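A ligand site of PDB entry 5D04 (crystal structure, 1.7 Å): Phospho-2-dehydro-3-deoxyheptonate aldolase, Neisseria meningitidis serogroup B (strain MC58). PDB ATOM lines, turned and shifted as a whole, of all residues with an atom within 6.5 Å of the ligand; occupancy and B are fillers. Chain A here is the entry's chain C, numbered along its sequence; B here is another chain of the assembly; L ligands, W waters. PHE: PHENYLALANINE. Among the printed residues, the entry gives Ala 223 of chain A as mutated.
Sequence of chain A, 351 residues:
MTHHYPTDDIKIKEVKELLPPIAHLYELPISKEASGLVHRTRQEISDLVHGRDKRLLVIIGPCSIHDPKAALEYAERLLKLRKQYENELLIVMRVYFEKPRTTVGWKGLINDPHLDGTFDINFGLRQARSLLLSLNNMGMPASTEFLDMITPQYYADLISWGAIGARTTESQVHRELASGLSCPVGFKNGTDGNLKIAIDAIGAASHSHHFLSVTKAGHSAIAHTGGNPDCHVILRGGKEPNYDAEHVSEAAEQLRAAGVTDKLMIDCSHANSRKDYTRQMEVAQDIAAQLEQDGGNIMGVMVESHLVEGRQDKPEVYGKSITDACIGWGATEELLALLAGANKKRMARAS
OE1 of Gln 153 is in hydrogen-bond range of N of the ligand. The side-chain carboxylate (OD1) of Asp 8 of chain B lies within salt-bridge range of a nitrogen (N) of the ligand, 3.5 Å away. The backbone NH (N) of Ser 182 is in hydrogen-bond range of an oxygen (O) of the ligand (2.8 Å). The side-chain hydroxyl (OG) of Ser 182 is in hydrogen-bond range of an oxygen (OXT) of the ligand (2.6 Å). The side-chain carboxylate (OD1) of Asp 9 of chain B is in salt-bridge range of a nitrogen (N) of the ligand, 2.7 Å away. The backbone NH of Asp 9 of chain B sits at hydrogen-bond distance from an oxygen (OXT) of the ligand.
The side-chain amino group (NZ) of Lys 216 sits at hydrogen-bond distance from the side-chain amide oxygen (OE1) of Gln 153, at 2.8 Å. O of Phe 211 is in hydrogen-bond range of N of Ala 223 (2.8 Å). The guanidinium group (NH2) of Arg 42 is in hydrogen-bond range of the backbone carbonyl oxygen (O) of Ala 156, 2.8 Å away. OG of Ser 213 sits at hydrogen-bond distance from O of Met 149 (2.7 Å). The side-chain hydroxyl of Ser 182 is in hydrogen-bond range of the backbone NH of Ile 10 of chain B (3.1 Å). The backbone carbonyl oxygen (O) of Ser 182 sits at hydrogen-bond distance from the side-chain amino group (NZ) of Lys 11 of chain B, at 3.2 Å. N of Asp 9 of chain B lies within hydrogen-bond range of OG of Ser 182, at 3.3 Å. The side-chain carboxylate of Asp 9 of chain B lies within salt-bridge range of the side-chain amino group of Lys 216, 3.5 Å away.
Residues that only touch the ligand: Met 149, Pro 152, Ala 156, Leu 177, Gly 180, Leu 181, Phe 211, Ser 213, Lys 216 and Ile 12 of chain B. The nearest printed residue that does not touch the ligand is Thr 7 of chain B (4.1 Å).
Water W1 lies within hydrogen-bond range of N of the ligand, OD1 of Asp 8 of chain B and N of Asp 157.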
ATOM      1  N   ARG A  42      15.659  11.535 -21.839  1.00  0.00           N
ATOM      2  CA  ARG A  42      16.120  11.521 -20.429  1.00  0.00           C
ATOM      3  C   ARG A  42      16.425  12.939 -19.921  1.00  0.00           C
ATOM      4  O   ARG A  42      16.037  13.302 -18.821  1.00  0.00           O
ATOM      5  CB  ARG A  42      17.327  10.639 -20.260  1.00  0.00           C
ATOM      6  CG  ARG A  42      17.003   9.153 -20.315  1.00  0.00           C
ATOM      7  CD  ARG A  42      18.259   8.307 -20.461  1.00  0.00           C
ATOM      8  NE  ARG A  42      17.966   6.873 -20.481  1.00  0.00           N
ATOM      9  CZ  ARG A  42      18.896   5.951 -20.668  1.00  0.00           C
ATOM     10  NH1 ARG A  42      20.149   6.321 -20.847  1.00  0.00           N
ATOM     11  NH2 ARG A  42      18.579   4.660 -20.643  1.00  0.00           N
ATOM     12  N   PHE A 146      10.835  -1.576 -13.694  1.00  0.00           N
ATOM     13  CA  PHE A 146      11.802  -2.638 -13.433  1.00  0.00           C
ATOM     14  C   PHE A 146      11.431  -3.356 -12.159  1.00  0.00           C
ATOM     15  O   PHE A 146      11.439  -2.776 -11.098  1.00  0.00           O
ATOM     16  CB  PHE A 146      13.227  -2.071 -13.364  1.00  0.00           C
ATOM     17  CG  PHE A 146      13.670  -1.382 -14.640  1.00  0.00           C
ATOM     18  CD1 PHE A 146      14.031  -2.102 -15.738  1.00  0.00           C
ATOM     19  CD2 PHE A 146      13.752   0.008 -14.691  1.00  0.00           C
ATOM     20  CE1 PHE A 146      14.466  -1.461 -16.893  1.00  0.00           C
ATOM     21  CE2 PHE A 146      14.168   0.662 -15.856  1.00  0.00           C
ATOM     22  CZ  PHE A 146      14.526  -0.091 -16.950  1.00  0.00           C
ATOM     23  N   MET A 149      16.438  -6.848 -10.520  1.00  0.00           N
ATOM     24  CA  MET A 149      17.734  -6.199 -10.651  1.00  0.00           C
ATOM     25  C   MET A 149      18.554  -6.719 -11.828  1.00  0.00           C
ATOM     26  O   MET A 149      19.674  -6.262 -12.060  1.00  0.00           O
ATOM     27  CB  MET A 149      18.532  -6.332  -9.312  1.00  0.00           C
ATOM     28  CG  MET A 149      18.223  -5.266  -8.280  1.00  0.00           C
ATOM     29  SD  MET A 149      16.484  -5.019  -7.819  1.00  0.00           S
ATOM     30  CE  MET A 149      16.110  -6.544  -7.049  1.00  0.00           C
ATOM     31  N   ILE A 150      17.986  -7.683 -12.561  1.00  0.00           N
ATOM     32  CA  ILE A 150      18.649  -8.333 -13.666  1.00  0.00           C
ATOM     33  C   ILE A 150      18.054  -7.871 -15.007  1.00  0.00           C
ATOM     34  O   ILE A 150      18.807  -7.585 -15.950  1.00  0.00           O
ATOM     35  CB  ILE A 150      18.574  -9.843 -13.465  1.00  0.00           C
ATOM     36  CG1 ILE A 150      19.472 -10.210 -12.277  1.00  0.00           C
ATOM     37  CG2 ILE A 150      18.937 -10.624 -14.737  1.00  0.00           C
ATOM     38  CD1 ILE A 150      19.326 -11.647 -11.812  1.00  0.00           C
ATOM     39  N   PRO A 152      17.002  -5.053 -16.100  1.00  0.00           N
ATOM     40  CA  PRO A 152      17.552  -3.822 -16.690  1.00  0.00           C
ATOM     41  C   PRO A 152      18.794  -4.040 -17.539  1.00  0.00           C
ATOM     42  O   PRO A 152      19.061  -3.284 -18.469  1.00  0.00           O
ATOM     43  CB  PRO A 152      17.915  -2.929 -15.472  1.00  0.00           C
ATOM     44  CG  PRO A 152      17.116  -3.508 -14.365  1.00  0.00           C
ATOM     45  CD  PRO A 152      16.925  -4.962 -14.616  1.00  0.00           C
ATOM     46  N   GLN A 153      19.595  -5.078 -17.261  1.00  0.00           N
ATOM     47  CA  GLN A 153      20.765  -5.275 -18.110  1.00  0.00           C
ATOM     48  C   GLN A 153      20.410  -5.618 -19.546  1.00  0.00           C
ATOM     49  O   GLN A 153      21.237  -5.413 -20.461  1.00  0.00           O
ATOM     50  CB  GLN A 153      21.709  -6.346 -17.519  1.00  0.00           C
ATOM     51  CG  GLN A 153      22.406  -5.886 -16.240  1.00  0.00           C
ATOM     52  CD  GLN A 153      23.507  -4.857 -16.490  1.00  0.00           C
ATOM     53  OE1 GLN A 153      23.247  -3.778 -17.073  1.00  0.00           O
ATOM     54  NE2 GLN A 153      24.754  -5.231 -16.202  1.00  0.00           N
ATOM     55  N   ALA A 156      17.631  -1.668 -20.426  1.00  0.00           N
ATOM     56  CA  ALA A 156      17.520  -0.337 -19.829  1.00  0.00           C
ATOM     57  C   ALA A 156      18.134   0.780 -20.691  1.00  0.00           C
ATOM     58  O   ALA A 156      17.773   1.965 -20.544  1.00  0.00           O
ATOM     59  CB  ALA A 156      18.144  -0.304 -18.461  1.00  0.00           C
ATOM     60  N   ASP A 157      19.051   0.416 -21.556  1.00  0.00           N
ATOM     61  CA  ASP A 157      19.682   1.332 -22.477  1.00  0.00           C
ATOM     62  C   ASP A 157      18.623   1.947 -23.427  1.00  0.00           C
ATOM     63  O   ASP A 157      18.879   2.994 -24.013  1.00  0.00           O
ATOM     64  CB  ASP A 157      20.819   0.692 -23.253  1.00  0.00           C
ATOM     65  CG  ASP A 157      20.365  -0.495 -24.105  1.00  0.00           C
ATOM     66  OD1 ASP A 157      19.630  -1.384 -23.580  1.00  0.00           O
ATOM     67  OD2 ASP A 157      20.707  -0.520 -25.315  1.00  0.00           O
ATOM     68  N   LEU A 177      18.861  -0.244  -6.950  1.00  0.00           N
ATOM     69  CA  LEU A 177      18.755  -0.333  -8.413  1.00  0.00           C
ATOM     70  C   LEU A 177      18.523   1.072  -9.031  1.00  0.00           C
ATOM     71  O   LEU A 177      19.245   1.519  -9.956  1.00  0.00           O
ATOM     72  CB  LEU A 177      17.650  -1.303  -8.820  1.00  0.00           C
ATOM     73  CG  LEU A 177      17.303  -1.278 -10.292  1.00  0.00           C
ATOM     74  CD1 LEU A 177      18.492  -1.735 -11.148  1.00  0.00           C
ATOM     75  CD2 LEU A 177      16.045  -2.102 -10.569  1.00  0.00           C
ATOM     76  N   GLY A 180      21.213   3.501  -9.692  1.00  0.00           N
ATOM     77  CA  GLY A 180      22.087   3.217 -10.817  1.00  0.00           C
ATOM     78  C   GLY A 180      21.384   3.142 -12.153  1.00  0.00           C
ATOM     79  O   GLY A 180      22.006   2.707 -13.111  1.00  0.00           O
ATOM     80  N   LEU A 181      20.124   3.526 -12.241  1.00  0.00           N
ATOM     81  CA  LEU A 181      19.444   3.447 -13.532  1.00  0.00           C
ATOM     82  C   LEU A 181      19.761   4.675 -14.359  1.00  0.00           C
ATOM     83  O   LEU A 181      19.787   5.815 -13.850  1.00  0.00           O
ATOM     84  CB  LEU A 181      17.943   3.312 -13.380  1.00  0.00           C
ATOM     85  CG  LEU A 181      17.441   1.901 -12.979  1.00  0.00           C
ATOM     86  CD1 LEU A 181      15.969   1.905 -12.634  1.00  0.00           C
ATOM     87  CD2 LEU A 181      17.688   0.899 -14.087  1.00  0.00           C
ATOM     88  N   SER A 182      19.999   4.441 -15.645  1.00  0.00           N
ATOM     89  CA  SER A 182      20.428   5.544 -16.538  1.00  0.00           C
ATOM     90  C   SER A 182      19.311   6.545 -16.780  1.00  0.00           C
ATOM     91  O   SER A 182      19.557   7.736 -17.091  1.00  0.00           O
ATOM     92  CB  SER A 182      20.905   4.992 -17.864  1.00  0.00           C
ATOM     93  OG  SER A 182      22.030   4.167 -17.680  1.00  0.00           O
ATOM     94  N   CYS A 183      18.073   6.076 -16.651  1.00  0.00           N
ATOM     95  CA  CYS A 183      16.888   6.949 -16.823  1.00  0.00           C
ATOM     96  C   CYS A 183      16.488   7.655 -15.516  1.00  0.00           C
ATOM     97  O   CYS A 183      16.844   7.212 -14.415  1.00  0.00           O
ATOM     98  CB  CYS A 183      15.706   6.109 -17.314  1.00  0.00           C
ATOM     99  SG  CYS A 183      15.314   4.708 -16.271  1.00  0.00           S
ATOM    100  N   PHE A 211      24.559  -3.150  -5.403  1.00  0.00           N
ATOM    101  CA  PHE A 211      23.583  -4.227  -5.394  1.00  0.00           C
ATOM    102  C   PHE A 211      24.096  -5.322  -6.324  1.00  0.00           C
ATOM    103  O   PHE A 211      24.909  -5.065  -7.203  1.00  0.00           O
ATOM    104  CB  PHE A 211      22.182  -3.745  -5.835  1.00  0.00           C
ATOM    105  CG  PHE A 211      22.098  -3.235  -7.271  1.00  0.00           C
ATOM    106  CD1 PHE A 211      22.372  -1.911  -7.570  1.00  0.00           C
ATOM    107  CD2 PHE A 211      21.751  -4.073  -8.328  1.00  0.00           C
ATOM    108  CE1 PHE A 211      22.332  -1.456  -8.894  1.00  0.00           C
ATOM    109  CE2 PHE A 211      21.694  -3.612  -9.640  1.00  0.00           C
ATOM    110  CZ  PHE A 211      21.964  -2.292  -9.926  1.00  0.00           C
ATOM    111  N   LEU A 212      23.556  -6.527  -6.148  1.00  0.00           N
ATOM    112  CA  LEU A 212      23.962  -7.674  -6.950  1.00  0.00           C
ATOM    113  C   LEU A 212      23.138  -7.833  -8.196  1.00  0.00           C
ATOM    114  O   LEU A 212      21.924  -7.590  -8.198  1.00  0.00           O
ATOM    115  CB  LEU A 212      23.919  -8.946  -6.136  1.00  0.00           C
ATOM    116  CG  LEU A 212      24.699  -8.940  -4.806  1.00  0.00           C
ATOM    117  CD1 LEU A 212      24.787 -10.362  -4.277  1.00  0.00           C
ATOM    118  CD2 LEU A 212      26.073  -8.346  -4.960  1.00  0.00           C
ATOM    119  N   SER A 213      23.805  -8.229  -9.274  1.00  0.00           N
ATOM    120  CA  SER A 213      23.124  -8.414 -10.561  1.00  0.00           C
ATOM    121  C   SER A 213      23.984  -9.334 -11.396  1.00  0.00           C
ATOM    122  O   SER A 213      24.707 -10.184 -10.851  1.00  0.00           O
ATOM    123  CB  SER A 213      22.896  -7.075 -11.237  1.00  0.00           C
ATOM    124  OG  SER A 213      22.131  -7.208 -12.426  1.00  0.00           O
ATOM    125  N   VAL A 214      23.950  -9.125 -12.703  1.00  0.00           N
ATOM    126  CA  VAL A 214      24.870  -9.802 -13.606  1.00  0.00           C
ATOM    127  C   VAL A 214      25.575  -8.778 -14.500  1.00  0.00           C
ATOM    128  O   VAL A 214      25.042  -7.712 -14.754  1.00  0.00           O
ATOM    129  CB  VAL A 214      24.180 -10.855 -14.498  1.00  0.00           C
ATOM    130  CG1 VAL A 214      23.615 -11.977 -13.653  1.00  0.00           C
ATOM    131  CG2 VAL A 214      23.113 -10.214 -15.364  1.00  0.00           C
ATOM    132  N   LYS A 216      27.020  -7.709 -18.314  1.00  0.00           N
ATOM    133  CA  LYS A 216      26.378  -7.865 -19.626  1.00  0.00           C
ATOM    134  C   LYS A 216      26.661  -9.273 -20.201  1.00  0.00           C
ATOM    135  O   LYS A 216      25.855  -9.806 -20.918  1.00  0.00           O
ATOM    136  CB  LYS A 216      26.815  -6.759 -20.594  1.00  0.00           C
ATOM    137  CG  LYS A 216      26.396  -5.345 -20.214  1.00  0.00           C
ATOM    138  CD  LYS A 216      24.887  -5.204 -20.139  1.00  0.00           C
ATOM    139  CE  LYS A 216      24.402  -3.779 -20.265  1.00  0.00           C
ATOM    140  NZ  LYS A 216      24.893  -2.929 -19.168  1.00  0.00           N
ATOM    141  N   ALA A 223      27.190  -4.320  -8.666  1.00  0.00           N
ATOM    142  CA  ALA A 223      27.111  -3.074  -9.372  1.00  0.00           C
ATOM    143  C   ALA A 223      27.299  -1.976  -8.314  1.00  0.00           C
ATOM    144  O   ALA A 223      26.678  -2.024  -7.254  1.00  0.00           O
ATOM    145  CB  ALA A 223      25.753  -2.943 -10.027  1.00  0.00           C
ATOM    146  N   THR B   7      23.920   5.655 -23.685  1.00  0.00           N
ATOM    147  CA  THR B   7      22.669   5.363 -22.985  1.00  0.00           C
ATOM    148  C   THR B   7      22.808   4.256 -21.915  1.00  0.00           C
ATOM    149  O   THR B   7      21.860   4.009 -21.207  1.00  0.00           O
ATOM    150  CB  THR B   7      21.573   4.876 -23.964  1.00  0.00           C
ATOM    151  OG1 THR B   7      22.038   3.688 -24.598  1.00  0.00           O
ATOM    152  CG2 THR B   7      21.279   5.980 -25.030  1.00  0.00           C
ATOM    153  N   ASP B   8      23.945   3.550 -21.844  1.00  0.00           N
ATOM    154  CA  ASP B   8      24.071   2.361 -20.982  1.00  0.00           C
ATOM    155  C   ASP B   8      24.997   2.701 -19.809  1.00  0.00           C
ATOM    156  O   ASP B   8      26.070   3.281 -20.001  1.00  0.00           O
ATOM    157  CB  ASP B   8      24.695   1.247 -21.814  1.00  0.00           C
ATOM    158  CG  ASP B   8      24.972  -0.021 -21.061  1.00  0.00           C
ATOM    159  OD1 ASP B   8      24.244  -0.411 -20.151  1.00  0.00           O
ATOM    160  OD2 ASP B   8      25.976  -0.674 -21.433  1.00  0.00           O
ATOM    161  N   ASP B   9      24.583   2.367 -18.597  1.00  0.00           N
ATOM    162  CA  ASP B   9      25.452   2.464 -17.419  1.00  0.00           C
ATOM    163  C   ASP B   9      25.925   3.898 -17.155  1.00  0.00           C
ATOM    164  O   ASP B   9      27.042   4.121 -16.672  1.00  0.00           O
ATOM    165  CB  ASP B   9      26.640   1.494 -17.540  1.00  0.00           C
ATOM    166  CG  ASP B   9      26.258   0.061 -17.201  1.00  0.00           C
ATOM    167  OD1 ASP B   9      25.058  -0.204 -16.949  1.00  0.00           O
ATOM    168  OD2 ASP B   9      27.178  -0.808 -17.188  1.00  0.00           O
ATOM    169  N   ILE B  10      25.040   4.845 -17.450  1.00  0.00           N
ATOM    170  CA  ILE B  10      25.319   6.274 -17.280  1.00  0.00           C
ATOM    171  C   ILE B  10      25.629   6.638 -15.813  1.00  0.00           C
ATOM    172  O   ILE B  10      26.493   7.480 -15.546  1.00  0.00           O
ATOM    173  CB  ILE B  10      24.119   7.108 -17.764  1.00  0.00           C
ATOM    174  CG1 ILE B  10      23.804   6.756 -19.236  1.00  0.00           C
ATOM    175  CG2 ILE B  10      24.383   8.605 -17.577  1.00  0.00           C
ATOM    176  CD1 ILE B  10      24.944   6.909 -20.201  1.00  0.00           C
ATOM    177  N   LYS B  11      24.929   6.012 -14.884  1.00  0.00           N
ATOM    178  CA  LYS B  11      25.040   6.265 -13.444  1.00  0.00           C
ATOM    179  C   LYS B  11      25.637   5.070 -12.707  1.00  0.00           C
ATOM    180  O   LYS B  11      25.323   4.832 -11.558  1.00  0.00           O
ATOM    181  CB  LYS B  11      23.679   6.673 -12.875  1.00  0.00           C
ATOM    182  CG  LYS B  11      23.006   7.783 -13.678  1.00  0.00           C
ATOM    183  CD  LYS B  11      21.674   8.289 -13.153  1.00  0.00           C
ATOM    184  CE  LYS B  11      20.877   9.005 -14.244  1.00  0.00           C
ATOM    185  NZ  LYS B  11      19.423   8.789 -14.096  1.00  0.00           N
ATOM    186  N   ILE B  12      26.480   4.312 -13.389  1.00  0.00           N
ATOM    187  CA  ILE B  12      27.197   3.193 -12.791  1.00  0.00           C
ATOM    188  C   ILE B  12      28.704   3.496 -12.741  1.00  0.00           C
ATOM    189  O   ILE B  12      29.308   3.915 -13.750  1.00  0.00           O
ATOM    190  CB  ILE B  12      26.999   1.947 -13.675  1.00  0.00           C
ATOM    191  CG1 ILE B  12      25.530   1.486 -13.616  1.00  0.00           C
ATOM    192  CG2 ILE B  12      27.968   0.844 -13.380  1.00  0.00           C
ATOM    193  CD1 ILE B  12      25.079   0.993 -12.264  1.00  0.00           C
ATOM    194  N   VAL B  15      30.746  -2.349 -12.709  1.00  0.00           N
ATOM    195  CA  VAL B  15      30.065  -3.595 -12.513  1.00  0.00           C
ATOM    196  C   VAL B  15      31.134  -4.661 -12.501  1.00  0.00           C
ATOM    197  O   VAL B  15      31.803  -4.878 -13.514  1.00  0.00           O
ATOM    198  CB  VAL B  15      29.033  -3.887 -13.611  1.00  0.00           C
ATOM    199  CG1 VAL B  15      28.373  -5.238 -13.411  1.00  0.00           C
ATOM    200  CG2 VAL B  15      27.955  -2.806 -13.637  1.00  0.00           C
HETATM  201  N   PHE L   1      22.442  -0.954 -17.234  1.00  0.00           N
HETATM  202  CA  PHE L   1      21.488  -0.217 -16.354  1.00  0.00           C
HETATM  203  C   PHE L   1      21.209   1.150 -16.922  1.00  0.00           C
HETATM  204  O   PHE L   1      20.252   1.797 -16.459  1.00  0.00           O
HETATM  205  CB  PHE L   1      22.050  -0.099 -14.925  1.00  0.00           C
HETATM  206  CG  PHE L   1      22.263  -1.421 -14.271  1.00  0.00           C
HETATM  207  CD1 PHE L   1      21.184  -2.162 -13.769  1.00  0.00           C
HETATM  208  CD2 PHE L   1      23.540  -1.966 -14.206  1.00  0.00           C
HETATM  209  CE1 PHE L   1      21.425  -3.417 -13.193  1.00  0.00           C
HETATM  210  CE2 PHE L   1      23.762  -3.182 -13.656  1.00  0.00           C
HETATM  211  CZ  PHE L   1      22.714  -3.921 -13.158  1.00  0.00           C
HETATM  212  OXT PHE L   1      21.931   1.585 -17.873  1.00  0.00           O
HETATM  213  O   HOH W   1      21.544  -1.169 -19.845  1.00  0.00           O
